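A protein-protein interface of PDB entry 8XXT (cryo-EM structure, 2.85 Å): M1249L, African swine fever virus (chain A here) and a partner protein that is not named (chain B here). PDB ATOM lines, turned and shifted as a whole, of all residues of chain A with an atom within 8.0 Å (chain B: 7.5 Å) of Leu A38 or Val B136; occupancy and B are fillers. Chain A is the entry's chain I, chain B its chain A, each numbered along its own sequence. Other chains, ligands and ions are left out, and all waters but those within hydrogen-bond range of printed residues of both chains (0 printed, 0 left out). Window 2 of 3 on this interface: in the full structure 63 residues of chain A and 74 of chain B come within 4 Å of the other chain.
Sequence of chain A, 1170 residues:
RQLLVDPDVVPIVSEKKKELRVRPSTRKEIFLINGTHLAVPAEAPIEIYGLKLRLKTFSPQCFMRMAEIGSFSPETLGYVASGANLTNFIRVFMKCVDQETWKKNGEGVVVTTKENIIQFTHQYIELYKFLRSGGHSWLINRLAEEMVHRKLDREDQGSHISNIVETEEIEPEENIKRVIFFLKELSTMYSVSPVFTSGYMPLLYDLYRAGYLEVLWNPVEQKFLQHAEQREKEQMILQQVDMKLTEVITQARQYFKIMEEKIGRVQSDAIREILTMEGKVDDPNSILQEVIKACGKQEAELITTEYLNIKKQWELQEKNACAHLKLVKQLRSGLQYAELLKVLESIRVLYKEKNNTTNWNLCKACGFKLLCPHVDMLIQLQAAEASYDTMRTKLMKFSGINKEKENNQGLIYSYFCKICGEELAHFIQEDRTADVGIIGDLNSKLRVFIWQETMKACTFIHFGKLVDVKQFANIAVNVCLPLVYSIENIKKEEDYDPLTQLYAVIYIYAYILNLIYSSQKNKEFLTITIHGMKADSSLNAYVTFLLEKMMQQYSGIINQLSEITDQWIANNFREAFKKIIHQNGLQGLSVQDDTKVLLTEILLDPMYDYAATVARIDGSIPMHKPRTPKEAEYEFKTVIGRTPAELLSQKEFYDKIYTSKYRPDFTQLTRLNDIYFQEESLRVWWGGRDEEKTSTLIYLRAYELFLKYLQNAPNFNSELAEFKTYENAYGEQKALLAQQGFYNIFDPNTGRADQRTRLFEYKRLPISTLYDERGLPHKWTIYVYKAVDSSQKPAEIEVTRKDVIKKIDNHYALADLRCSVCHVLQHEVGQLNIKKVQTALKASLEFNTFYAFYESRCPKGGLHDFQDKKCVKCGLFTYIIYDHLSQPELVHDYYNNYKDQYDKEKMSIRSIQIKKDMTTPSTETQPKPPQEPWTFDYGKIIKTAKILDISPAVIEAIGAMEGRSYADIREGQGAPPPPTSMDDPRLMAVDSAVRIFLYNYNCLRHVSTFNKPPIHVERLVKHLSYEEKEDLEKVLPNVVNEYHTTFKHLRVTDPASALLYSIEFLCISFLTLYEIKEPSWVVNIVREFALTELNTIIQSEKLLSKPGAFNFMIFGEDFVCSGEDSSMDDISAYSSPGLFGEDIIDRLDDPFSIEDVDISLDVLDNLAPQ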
ATOM      1  N   VAL A  13      27.239  15.860 -34.200  1.00  0.00           N
ATOM      2  CA  VAL A  13      25.892  15.550 -34.663  1.00  0.00           C
ATOM      3  C   VAL A  13      25.155  16.839 -35.001  1.00  0.00           C
ATOM      4  O   VAL A  13      25.290  17.854 -34.307  1.00  0.00           O
ATOM      5  CB  VAL A  13      25.147  14.730 -33.592  1.00  0.00           C
ATOM      6  CG1 VAL A  13      23.639  14.832 -33.757  1.00  0.00           C
ATOM      7  CG2 VAL A  13      25.595  13.287 -33.638  1.00  0.00           C
ATOM      8  N   ARG A  27      31.373   1.468 -34.155  1.00  0.00           N
ATOM      9  CA  ARG A  27      30.933   2.417 -33.144  1.00  0.00           C
ATOM     10  C   ARG A  27      31.970   3.522 -32.979  1.00  0.00           C
ATOM     11  O   ARG A  27      33.103   3.272 -32.557  1.00  0.00           O
ATOM     12  CB  ARG A  27      30.682   1.692 -31.818  1.00  0.00           C
ATOM     13  CG  ARG A  27      30.454   2.558 -30.561  1.00  0.00           C
ATOM     14  CD  ARG A  27      29.762   3.907 -30.788  1.00  0.00           C
ATOM     15  NE  ARG A  27      28.563   3.833 -31.613  1.00  0.00           N
ATOM     16  CZ  ARG A  27      27.793   4.875 -31.889  1.00  0.00           C
ATOM     17  NH1 ARG A  27      28.058   6.077 -31.404  1.00  0.00           N
ATOM     18  NH2 ARG A  27      26.729   4.709 -32.667  1.00  0.00           N
ATOM     19  N   LYS A  28      31.567   4.744 -33.312  1.00  0.00           N
ATOM     20  CA  LYS A  28      32.391   5.931 -33.155  1.00  0.00           C
ATOM     21  C   LYS A  28      31.705   6.897 -32.200  1.00  0.00           C
ATOM     22  O   LYS A  28      30.526   7.219 -32.370  1.00  0.00           O
ATOM     23  CB  LYS A  28      32.633   6.606 -34.506  1.00  0.00           C
ATOM     24  CG  LYS A  28      33.461   7.867 -34.427  1.00  0.00           C
ATOM     25  CD  LYS A  28      34.880   7.546 -34.021  1.00  0.00           C
ATOM     26  CE  LYS A  28      35.686   7.094 -35.220  1.00  0.00           C
ATOM     27  NZ  LYS A  28      37.026   6.598 -34.831  1.00  0.00           N
ATOM     28  N   GLU A  29      32.442   7.355 -31.191  1.00  0.00           N
ATOM     29  CA  GLU A  29      31.892   8.298 -30.227  1.00  0.00           C
ATOM     30  C   GLU A  29      31.678   9.642 -30.909  1.00  0.00           C
ATOM     31  O   GLU A  29      32.579  10.155 -31.581  1.00  0.00           O
ATOM     32  CB  GLU A  29      32.819   8.443 -29.024  1.00  0.00           C
ATOM     33  CG  GLU A  29      32.114   8.902 -27.760  1.00  0.00           C
ATOM     34  CD  GLU A  29      33.056   9.551 -26.771  1.00  0.00           C
ATOM     35  OE1 GLU A  29      33.507  10.684 -27.035  1.00  0.00           O
ATOM     36  OE2 GLU A  29      33.351   8.924 -25.733  1.00  0.00           O
ATOM     37  N   ILE A  30      30.490  10.214 -30.734  1.00  0.00           N
ATOM     38  CA  ILE A  30      30.116  11.450 -31.402  1.00  0.00           C
ATOM     39  C   ILE A  30      29.755  12.501 -30.360  1.00  0.00           C
ATOM     40  O   ILE A  30      29.519  12.200 -29.189  1.00  0.00           O
ATOM     41  CB  ILE A  30      28.972  11.228 -32.426  1.00  0.00           C
ATOM     42  CG1 ILE A  30      27.722  10.578 -31.804  1.00  0.00           C
ATOM     43  CG2 ILE A  30      29.459  10.379 -33.589  1.00  0.00           C
ATOM     44  CD1 ILE A  30      26.883  11.439 -30.886  1.00  0.00           C
ATOM     45  N   PHE A  31      29.722  13.751 -30.809  1.00  0.00           N
ATOM     46  CA  PHE A  31      29.403  14.887 -29.960  1.00  0.00           C
ATOM     47  C   PHE A  31      28.180  15.618 -30.494  1.00  0.00           C
ATOM     48  O   PHE A  31      28.034  15.803 -31.705  1.00  0.00           O
ATOM     49  CB  PHE A  31      30.581  15.860 -29.883  1.00  0.00           C
ATOM     50  CG  PHE A  31      31.573  15.529 -28.812  1.00  0.00           C
ATOM     51  CD1 PHE A  31      32.383  14.414 -28.919  1.00  0.00           C
ATOM     52  CD2 PHE A  31      31.708  16.346 -27.703  1.00  0.00           C
ATOM     53  CE1 PHE A  31      33.303  14.115 -27.936  1.00  0.00           C
ATOM     54  CE2 PHE A  31      32.624  16.052 -26.718  1.00  0.00           C
ATOM     55  CZ  PHE A  31      33.424  14.937 -26.835  1.00  0.00           C
ATOM     56  N   LEU A  32      27.302  16.023 -29.586  1.00  0.00           N
ATOM     57  CA  LEU A  32      26.247  16.950 -29.953  1.00  0.00           C
ATOM     58  C   LEU A  32      26.831  18.347 -30.139  1.00  0.00           C
ATOM     59  O   LEU A  32      27.895  18.681 -29.610  1.00  0.00           O
ATOM     60  CB  LEU A  32      25.150  16.968 -28.889  1.00  0.00           C
ATOM     61  CG  LEU A  32      23.840  16.267 -29.249  1.00  0.00           C
ATOM     62  CD1 LEU A  32      22.856  16.348 -28.097  1.00  0.00           C
ATOM     63  CD2 LEU A  32      23.242  16.874 -30.506  1.00  0.00           C
ATOM     64  N   GLY A  35      27.715  20.230 -27.072  1.00  0.00           N
ATOM     65  CA  GLY A  35      28.840  19.800 -26.271  1.00  0.00           C
ATOM     66  C   GLY A  35      28.539  18.686 -25.295  1.00  0.00           C
ATOM     67  O   GLY A  35      29.396  18.371 -24.459  1.00  0.00           O
ATOM     68  N   THR A  36      27.359  18.083 -25.368  1.00  0.00           N
ATOM     69  CA  THR A  36      26.964  17.000 -24.482  1.00  0.00           C
ATOM     70  C   THR A  36      27.088  15.662 -25.202  1.00  0.00           C
ATOM     71  O   THR A  36      27.296  15.594 -26.416  1.00  0.00           O
ATOM     72  CB  THR A  36      25.531  17.205 -23.973  1.00  0.00           C
ATOM     73  OG1 THR A  36      24.655  17.435 -25.084  1.00  0.00           O
ATOM     74  CG2 THR A  36      25.469  18.396 -23.029  1.00  0.00           C
ATOM     75  N   HIS A  37      26.948  14.588 -24.430  1.00  0.00           N
ATOM     76  CA  HIS A  37      27.171  13.231 -24.910  1.00  0.00           C
ATOM     77  C   HIS A  37      25.853  12.470 -24.974  1.00  0.00           C
ATOM     78  O   HIS A  37      25.140  12.371 -23.970  1.00  0.00           O
ATOM     79  CB  HIS A  37      28.152  12.490 -24.003  1.00  0.00           C
ATOM     80  CG  HIS A  37      29.581  12.614 -24.425  1.00  0.00           C
ATOM     81  ND1 HIS A  37      30.630  12.453 -23.546  1.00  0.00           N
ATOM     82  CD2 HIS A  37      30.136  12.861 -25.633  1.00  0.00           C
ATOM     83  CE1 HIS A  37      31.771  12.607 -24.193  1.00  0.00           C
ATOM     84  NE2 HIS A  37      31.499  12.854 -25.462  1.00  0.00           N
ATOM     85  N   LEU A  38      25.542  11.940 -26.155  1.00  0.00           N
ATOM     86  CA  LEU A  38      24.540  10.897 -26.325  1.00  0.00           C
ATOM     87  C   LEU A  38      24.764  10.271 -27.693  1.00  0.00           C
ATOM     88  O   LEU A  38      24.740  10.965 -28.711  1.00  0.00           O
ATOM     89  CB  LEU A  38      23.103  11.428 -26.180  1.00  0.00           C
ATOM     90  CG  LEU A  38      22.550  12.566 -27.044  1.00  0.00           C
ATOM     91  CD1 LEU A  38      21.813  12.033 -28.267  1.00  0.00           C
ATOM     92  CD2 LEU A  38      21.642  13.460 -26.217  1.00  0.00           C
ATOM     93  N   ALA A  39      24.990   8.963 -27.704  1.00  0.00           N
ATOM     94  CA  ALA A  39      25.356   8.221 -28.902  1.00  0.00           C
ATOM     95  C   ALA A  39      24.133   7.522 -29.489  1.00  0.00           C
ATOM     96  O   ALA A  39      22.993   7.742 -29.068  1.00  0.00           O
ATOM     97  CB  ALA A  39      26.466   7.214 -28.591  1.00  0.00           C
ATOM     98  N   VAL A  40      24.382   6.687 -30.491  1.00  0.00           N
ATOM     99  CA  VAL A  40      23.343   5.887 -31.135  1.00  0.00           C
ATOM    100  C   VAL A  40      23.895   4.482 -31.347  1.00  0.00           C
ATOM    101  O   VAL A  40      25.072   4.237 -31.044  1.00  0.00           O
ATOM    102  CB  VAL A  40      22.895   6.512 -32.465  1.00  0.00           C
ATOM    103  CG1 VAL A  40      22.052   7.759 -32.220  1.00  0.00           C
ATOM    104  CG2 VAL A  40      24.104   6.833 -33.330  1.00  0.00           C
ATOM    105  N   ILE A  46      23.389   8.900 -38.971  1.00  0.00           N
ATOM    106  CA  ILE A  46      23.429  10.214 -38.358  1.00  0.00           C
ATOM    107  C   ILE A  46      23.947  11.229 -39.365  1.00  0.00           C
ATOM    108  O   ILE A  46      24.878  10.960 -40.129  1.00  0.00           O
ATOM    109  CB  ILE A  46      24.307  10.207 -37.088  1.00  0.00           C
ATOM    110  CG1 ILE A  46      23.757   9.206 -36.077  1.00  0.00           C
ATOM    111  CG2 ILE A  46      24.357  11.582 -36.466  1.00  0.00           C
ATOM    112  CD1 ILE A  46      22.276   9.381 -35.784  1.00  0.00           C
ATOM    113  N   CYS B  99      20.394   5.227 -19.932  1.00  0.00           N
ATOM    114  CA  CYS B  99      19.175   5.502 -20.678  1.00  0.00           C
ATOM    115  C   CYS B  99      19.109   4.573 -21.879  1.00  0.00           C
ATOM    116  O   CYS B  99      20.034   4.539 -22.697  1.00  0.00           O
ATOM    117  CB  CYS B  99      19.135   6.963 -21.119  1.00  0.00           C
ATOM    118  SG  CYS B  99      17.668   7.423 -22.063  1.00  0.00           S
ATOM    119  N   ASN B 101      17.517   4.792 -24.496  1.00  0.00           N
ATOM    120  CA  ASN B 101      17.308   5.464 -25.771  1.00  0.00           C
ATOM    121  C   ASN B 101      18.480   6.332 -26.203  1.00  0.00           C
ATOM    122  O   ASN B 101      18.707   6.484 -27.406  1.00  0.00           O
ATOM    123  CB  ASN B 101      16.045   6.326 -25.714  1.00  0.00           C
ATOM    124  CG  ASN B 101      14.780   5.500 -25.761  1.00  0.00           C
ATOM    125  OD1 ASN B 101      14.474   4.871 -26.771  1.00  0.00           O
ATOM    126  ND2 ASN B 101      14.036   5.493 -24.661  1.00  0.00           N
ATOM    127  N   CYS B 102      19.229   6.911 -25.264  1.00  0.00           N
ATOM    128  CA  CYS B 102      20.323   7.802 -25.618  1.00  0.00           C
ATOM    129  C   CYS B 102      21.669   7.397 -25.032  1.00  0.00           C
ATOM    130  O   CYS B 102      22.672   8.058 -25.322  1.00  0.00           O
ATOM    131  CB  CYS B 102      20.005   9.238 -25.187  1.00  0.00           C
ATOM    132  SG  CYS B 102      20.494   9.607 -23.502  1.00  0.00           S
ATOM    133  N   GLY B 103      21.725   6.340 -24.219  1.00  0.00           N
ATOM    134  CA  GLY B 103      22.973   5.853 -23.678  1.00  0.00           C
ATOM    135  C   GLY B 103      23.537   6.637 -22.515  1.00  0.00           C
ATOM    136  O   GLY B 103      24.352   6.095 -21.761  1.00  0.00           O
ATOM    137  N   ALA B 104      23.144   7.896 -22.341  1.00  0.00           N
ATOM    138  CA  ALA B 104      23.633   8.672 -21.217  1.00  0.00           C
ATOM    139  C   ALA B 104      23.095   8.101 -19.907  1.00  0.00           C
ATOM    140  O   ALA B 104      21.978   7.582 -19.858  1.00  0.00           O
ATOM    141  CB  ALA B 104      23.226  10.135 -21.354  1.00  0.00           C
ATOM    142  N   PRO B 105      23.876   8.175 -18.831  1.00  0.00           N
ATOM    143  CA  PRO B 105      23.419   7.607 -17.559  1.00  0.00           C
ATOM    144  C   PRO B 105      22.235   8.375 -16.998  1.00  0.00           C
ATOM    145  O   PRO B 105      22.195   9.607 -17.036  1.00  0.00           O
ATOM    146  CB  PRO B 105      24.649   7.735 -16.654  1.00  0.00           C
ATOM    147  CG  PRO B 105      25.392   8.896 -17.218  1.00  0.00           C
ATOM    148  CD  PRO B 105      25.189   8.830 -18.703  1.00  0.00           C
ATOM    149  N   GLN B 133      13.199  10.446 -15.774  1.00  0.00           N
ATOM    150  CA  GLN B 133      13.182  11.196 -17.022  1.00  0.00           C
ATOM    151  C   GLN B 133      14.602  11.591 -17.403  1.00  0.00           C
ATOM    152  O   GLN B 133      15.297  12.256 -16.628  1.00  0.00           O
ATOM    153  CB  GLN B 133      12.302  12.438 -16.888  1.00  0.00           C
ATOM    154  CG  GLN B 133      11.737  12.950 -18.201  1.00  0.00           C
ATOM    155  CD  GLN B 133      11.448  11.835 -19.183  1.00  0.00           C
ATOM    156  OE1 GLN B 133      12.228  11.584 -20.097  1.00  0.00           O
ATOM    157  NE2 GLN B 133      10.319  11.160 -19.000  1.00  0.00           N
ATOM    158  N   CYS B 134      15.028  11.180 -18.594  1.00  0.00           N
ATOM    159  CA  CYS B 134      16.381  11.477 -19.040  1.00  0.00           C
ATOM    160  C   CYS B 134      16.531  12.959 -19.360  1.00  0.00           C
ATOM    161  O   CYS B 134      15.650  13.575 -19.964  1.00  0.00           O
ATOM    162  CB  CYS B 134      16.733  10.641 -20.265  1.00  0.00           C
ATOM    163  SG  CYS B 134      18.315  11.082 -20.990  1.00  0.00           S
ATOM    164  N   TYR B 135      17.666  13.529 -18.955  1.00  0.00           N
ATOM    165  CA  TYR B 135      17.873  14.967 -19.091  1.00  0.00           C
ATOM    166  C   TYR B 135      18.221  15.367 -20.518  1.00  0.00           C
ATOM    167  O   TYR B 135      17.823  16.444 -20.973  1.00  0.00           O
ATOM    168  CB  TYR B 135      18.972  15.432 -18.136  1.00  0.00           C
ATOM    169  CG  TYR B 135      19.133  14.560 -16.911  1.00  0.00           C
ATOM    170  CD1 TYR B 135      18.099  14.414 -15.995  1.00  0.00           C
ATOM    171  CD2 TYR B 135      20.324  13.890 -16.667  1.00  0.00           C
ATOM    172  CE1 TYR B 135      18.244  13.618 -14.876  1.00  0.00           C
ATOM    173  CE2 TYR B 135      20.479  13.094 -15.549  1.00  0.00           C
ATOM    174  CZ  TYR B 135      19.436  12.963 -14.658  1.00  0.00           C
ATOM    175  OH  TYR B 135      19.588  12.170 -13.545  1.00  0.00           O
ATOM    176  N   VAL B 136      18.965  14.527 -21.237  1.00  0.00           N
ATOM    177  CA  VAL B 136      19.516  14.943 -22.522  1.00  0.00           C
ATOM    178  C   VAL B 136      18.669  14.523 -23.718  1.00  0.00           C
ATOM    179  O   VAL B 136      18.825  15.099 -24.804  1.00  0.00           O
ATOM    180  CB  VAL B 136      20.948  14.408 -22.701  1.00  0.00           C
ATOM    181  CG1 VAL B 136      21.938  15.312 -21.987  1.00  0.00           C
ATOM    182  CG2 VAL B 136      21.049  12.989 -22.185  1.00  0.00           C
ATOM    183  N   CYS B 137      17.785  13.540 -23.560  1.00  0.00           N
ATOM    184  CA  CYS B 137      16.939  13.112 -24.662  1.00  0.00           C
ATOM    185  C   CYS B 137      15.467  13.006 -24.292  1.00  0.00           C
ATOM    186  O   CYS B 137      14.657  12.651 -25.155  1.00  0.00           O
ATOM    187  CB  CYS B 137      17.425  11.769 -25.228  1.00  0.00           C
ATOM    188  SG  CYS B 137      16.819  10.310 -24.370  1.00  0.00           S
ATOM    189  N   LYS B 138      15.102  13.300 -23.043  1.00  0.00           N
ATOM    190  CA  LYS B 138      13.702  13.390 -22.623  1.00  0.00           C
ATOM    191  C   LYS B 138      12.939  12.098 -22.903  1.00  0.00           C
ATOM    192  O   LYS B 138      11.777  12.119 -23.315  1.00  0.00           O
ATOM    193  CB  LYS B 138      13.007  14.582 -23.286  1.00  0.00           C
ATOM    194  CG  LYS B 138      13.670  15.930 -23.027  1.00  0.00           C
ATOM    195  CD  LYS B 138      14.198  16.042 -21.603  1.00  0.00           C
ATOM    196  CE  LYS B 138      13.839  17.380 -20.977  1.00  0.00           C
ATOM    197  NZ  LYS B 138      14.768  17.739 -19.872  1.00  0.00           N
ATOM    198  N   ALA B 139      13.591  10.961 -22.675  1.00  0.00           N
ATOM    199  CA  ALA B 139      12.962   9.654 -22.797  1.00  0.00           C
ATOM    200  C   ALA B 139      12.902   9.000 -21.424  1.00  0.00           C
ATOM    201  O   ALA B 139      13.906   8.967 -20.705  1.00  0.00           O
ATOM    202  CB  ALA B 139      13.722   8.761 -23.777  1.00  0.00           C
ATOM    203  N   ARG B 176      25.555   2.196 -27.216  1.00  0.00           N
ATOM    204  CA  ARG B 176      25.263   3.612 -27.040  1.00  0.00           C
ATOM    205  C   ARG B 176      26.033   4.230 -25.878  1.00  0.00           C
ATOM    206  O   ARG B 176      26.101   5.459 -25.784  1.00  0.00           O
ATOM    207  CB  ARG B 176      23.762   3.812 -26.831  1.00  0.00           C
ATOM    208  CG  ARG B 176      23.257   5.171 -27.269  1.00  0.00           C
ATOM    209  CD  ARG B 176      21.764   5.170 -27.533  1.00  0.00           C
ATOM    210  NE  ARG B 176      21.321   3.990 -28.263  1.00  0.00           N
ATOM    211  CZ  ARG B 176      20.382   3.156 -27.840  1.00  0.00           C
ATOM    212  NH1 ARG B 176      19.764   3.339 -26.686  1.00  0.00           N
ATOM    213  NH2 ARG B 176      20.052   2.113 -28.596  1.00  0.00           N
ATOM    214  N   THR B 178      29.055   5.561 -23.603  1.00  0.00           N
ATOM    215  CA  THR B 178      30.373   6.135 -23.817  1.00  0.00           C
ATOM    216  C   THR B 178      31.344   5.670 -22.737  1.00  0.00           C
ATOM    217  O   THR B 178      30.949   5.146 -21.694  1.00  0.00           O
ATOM    218  CB  THR B 178      30.304   7.661 -23.829  1.00  0.00           C
ATOM    219  OG1 THR B 178      31.626   8.200 -23.718  1.00  0.00           O
ATOM    220  CG2 THR B 178      29.463   8.159 -22.669  1.00  0.00           C
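The side-chain carboxylate (OE2) of Glu A29 is in hydrogen-bond range of the side-chain hydroxyl (OG1) of Thr B178.
N of Ala A39 lies within hydrogen-bond range of O of Cys B102.
N of Cys B99 sits at hydrogen-bond distance from O of Ala B104 (2.8 Å).
N of Val B136 lies close to SG of Cys B134.
The backbone carbonyl oxygen (O) of Asn B101 sits close to the guanidinium group (NH1) of Arg B176, at 3.4 Å.
NE2 of His A37 is in hydrogen-bond range of OE1 of Glu A29 (3.3 Å).
The backbone NH (N) of Ala B104 lies close to the side-chain sulfur (SG) of Cys B102 (3.4 Å).
Among the printed residues, pairs that only touch across the chains: His A37 with Ala B104 (3.9 Å), Leu A38 with Cys B102 (3.5 Å), Leu A38 with Val B136 (3.6 Å), Ala A39 with Arg B176 (3.1 Å) and Val A40 with Arg B176 (3.7 Å).
Lys A28 touches none of the printed residues of chain B.
Printed residues of chain B within 4 Å of Glu A29: Thr B178 (2.7 Å).
Printed residues of chain B within 4 Å of His A37: Ala B104.
Leu A38 touches just these residues of chain B: Cys B102 (3.5 Å) and Val B136 (3.6 Å).
Printed residues of chain B within 4 Å of Val A40: Arg B176.
Of the printed residues of chain A, Ala B104 touches His A37.
Gln B133 touches none of the printed residues of chain A.
Of chain A, only Leu A38 comes within 4 Å of Val B136.
The nearest printed residue of chain A that does not touch Val B136 is His A37 (4.5 Å).
Of the 14 printed residues of chain A, 5 touch a printed residue of chain B.
Hydrophobic or aromatic side chains of chain A that line the printed part of chain B: Leu A38 and Ala A39.
Of the 15 printed residues of chain B, 5 touch a printed residue of chain A.
Printed residues of chain B that touch a printed residue of chain A: Cys B102, Ala B104, Val B136, Arg B176 and Thr B178.
Among the printed residues, no Asp or Glu carboxylate lies within 4 Å of a Lys or Arg side-chain nitrogen of the other chain.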
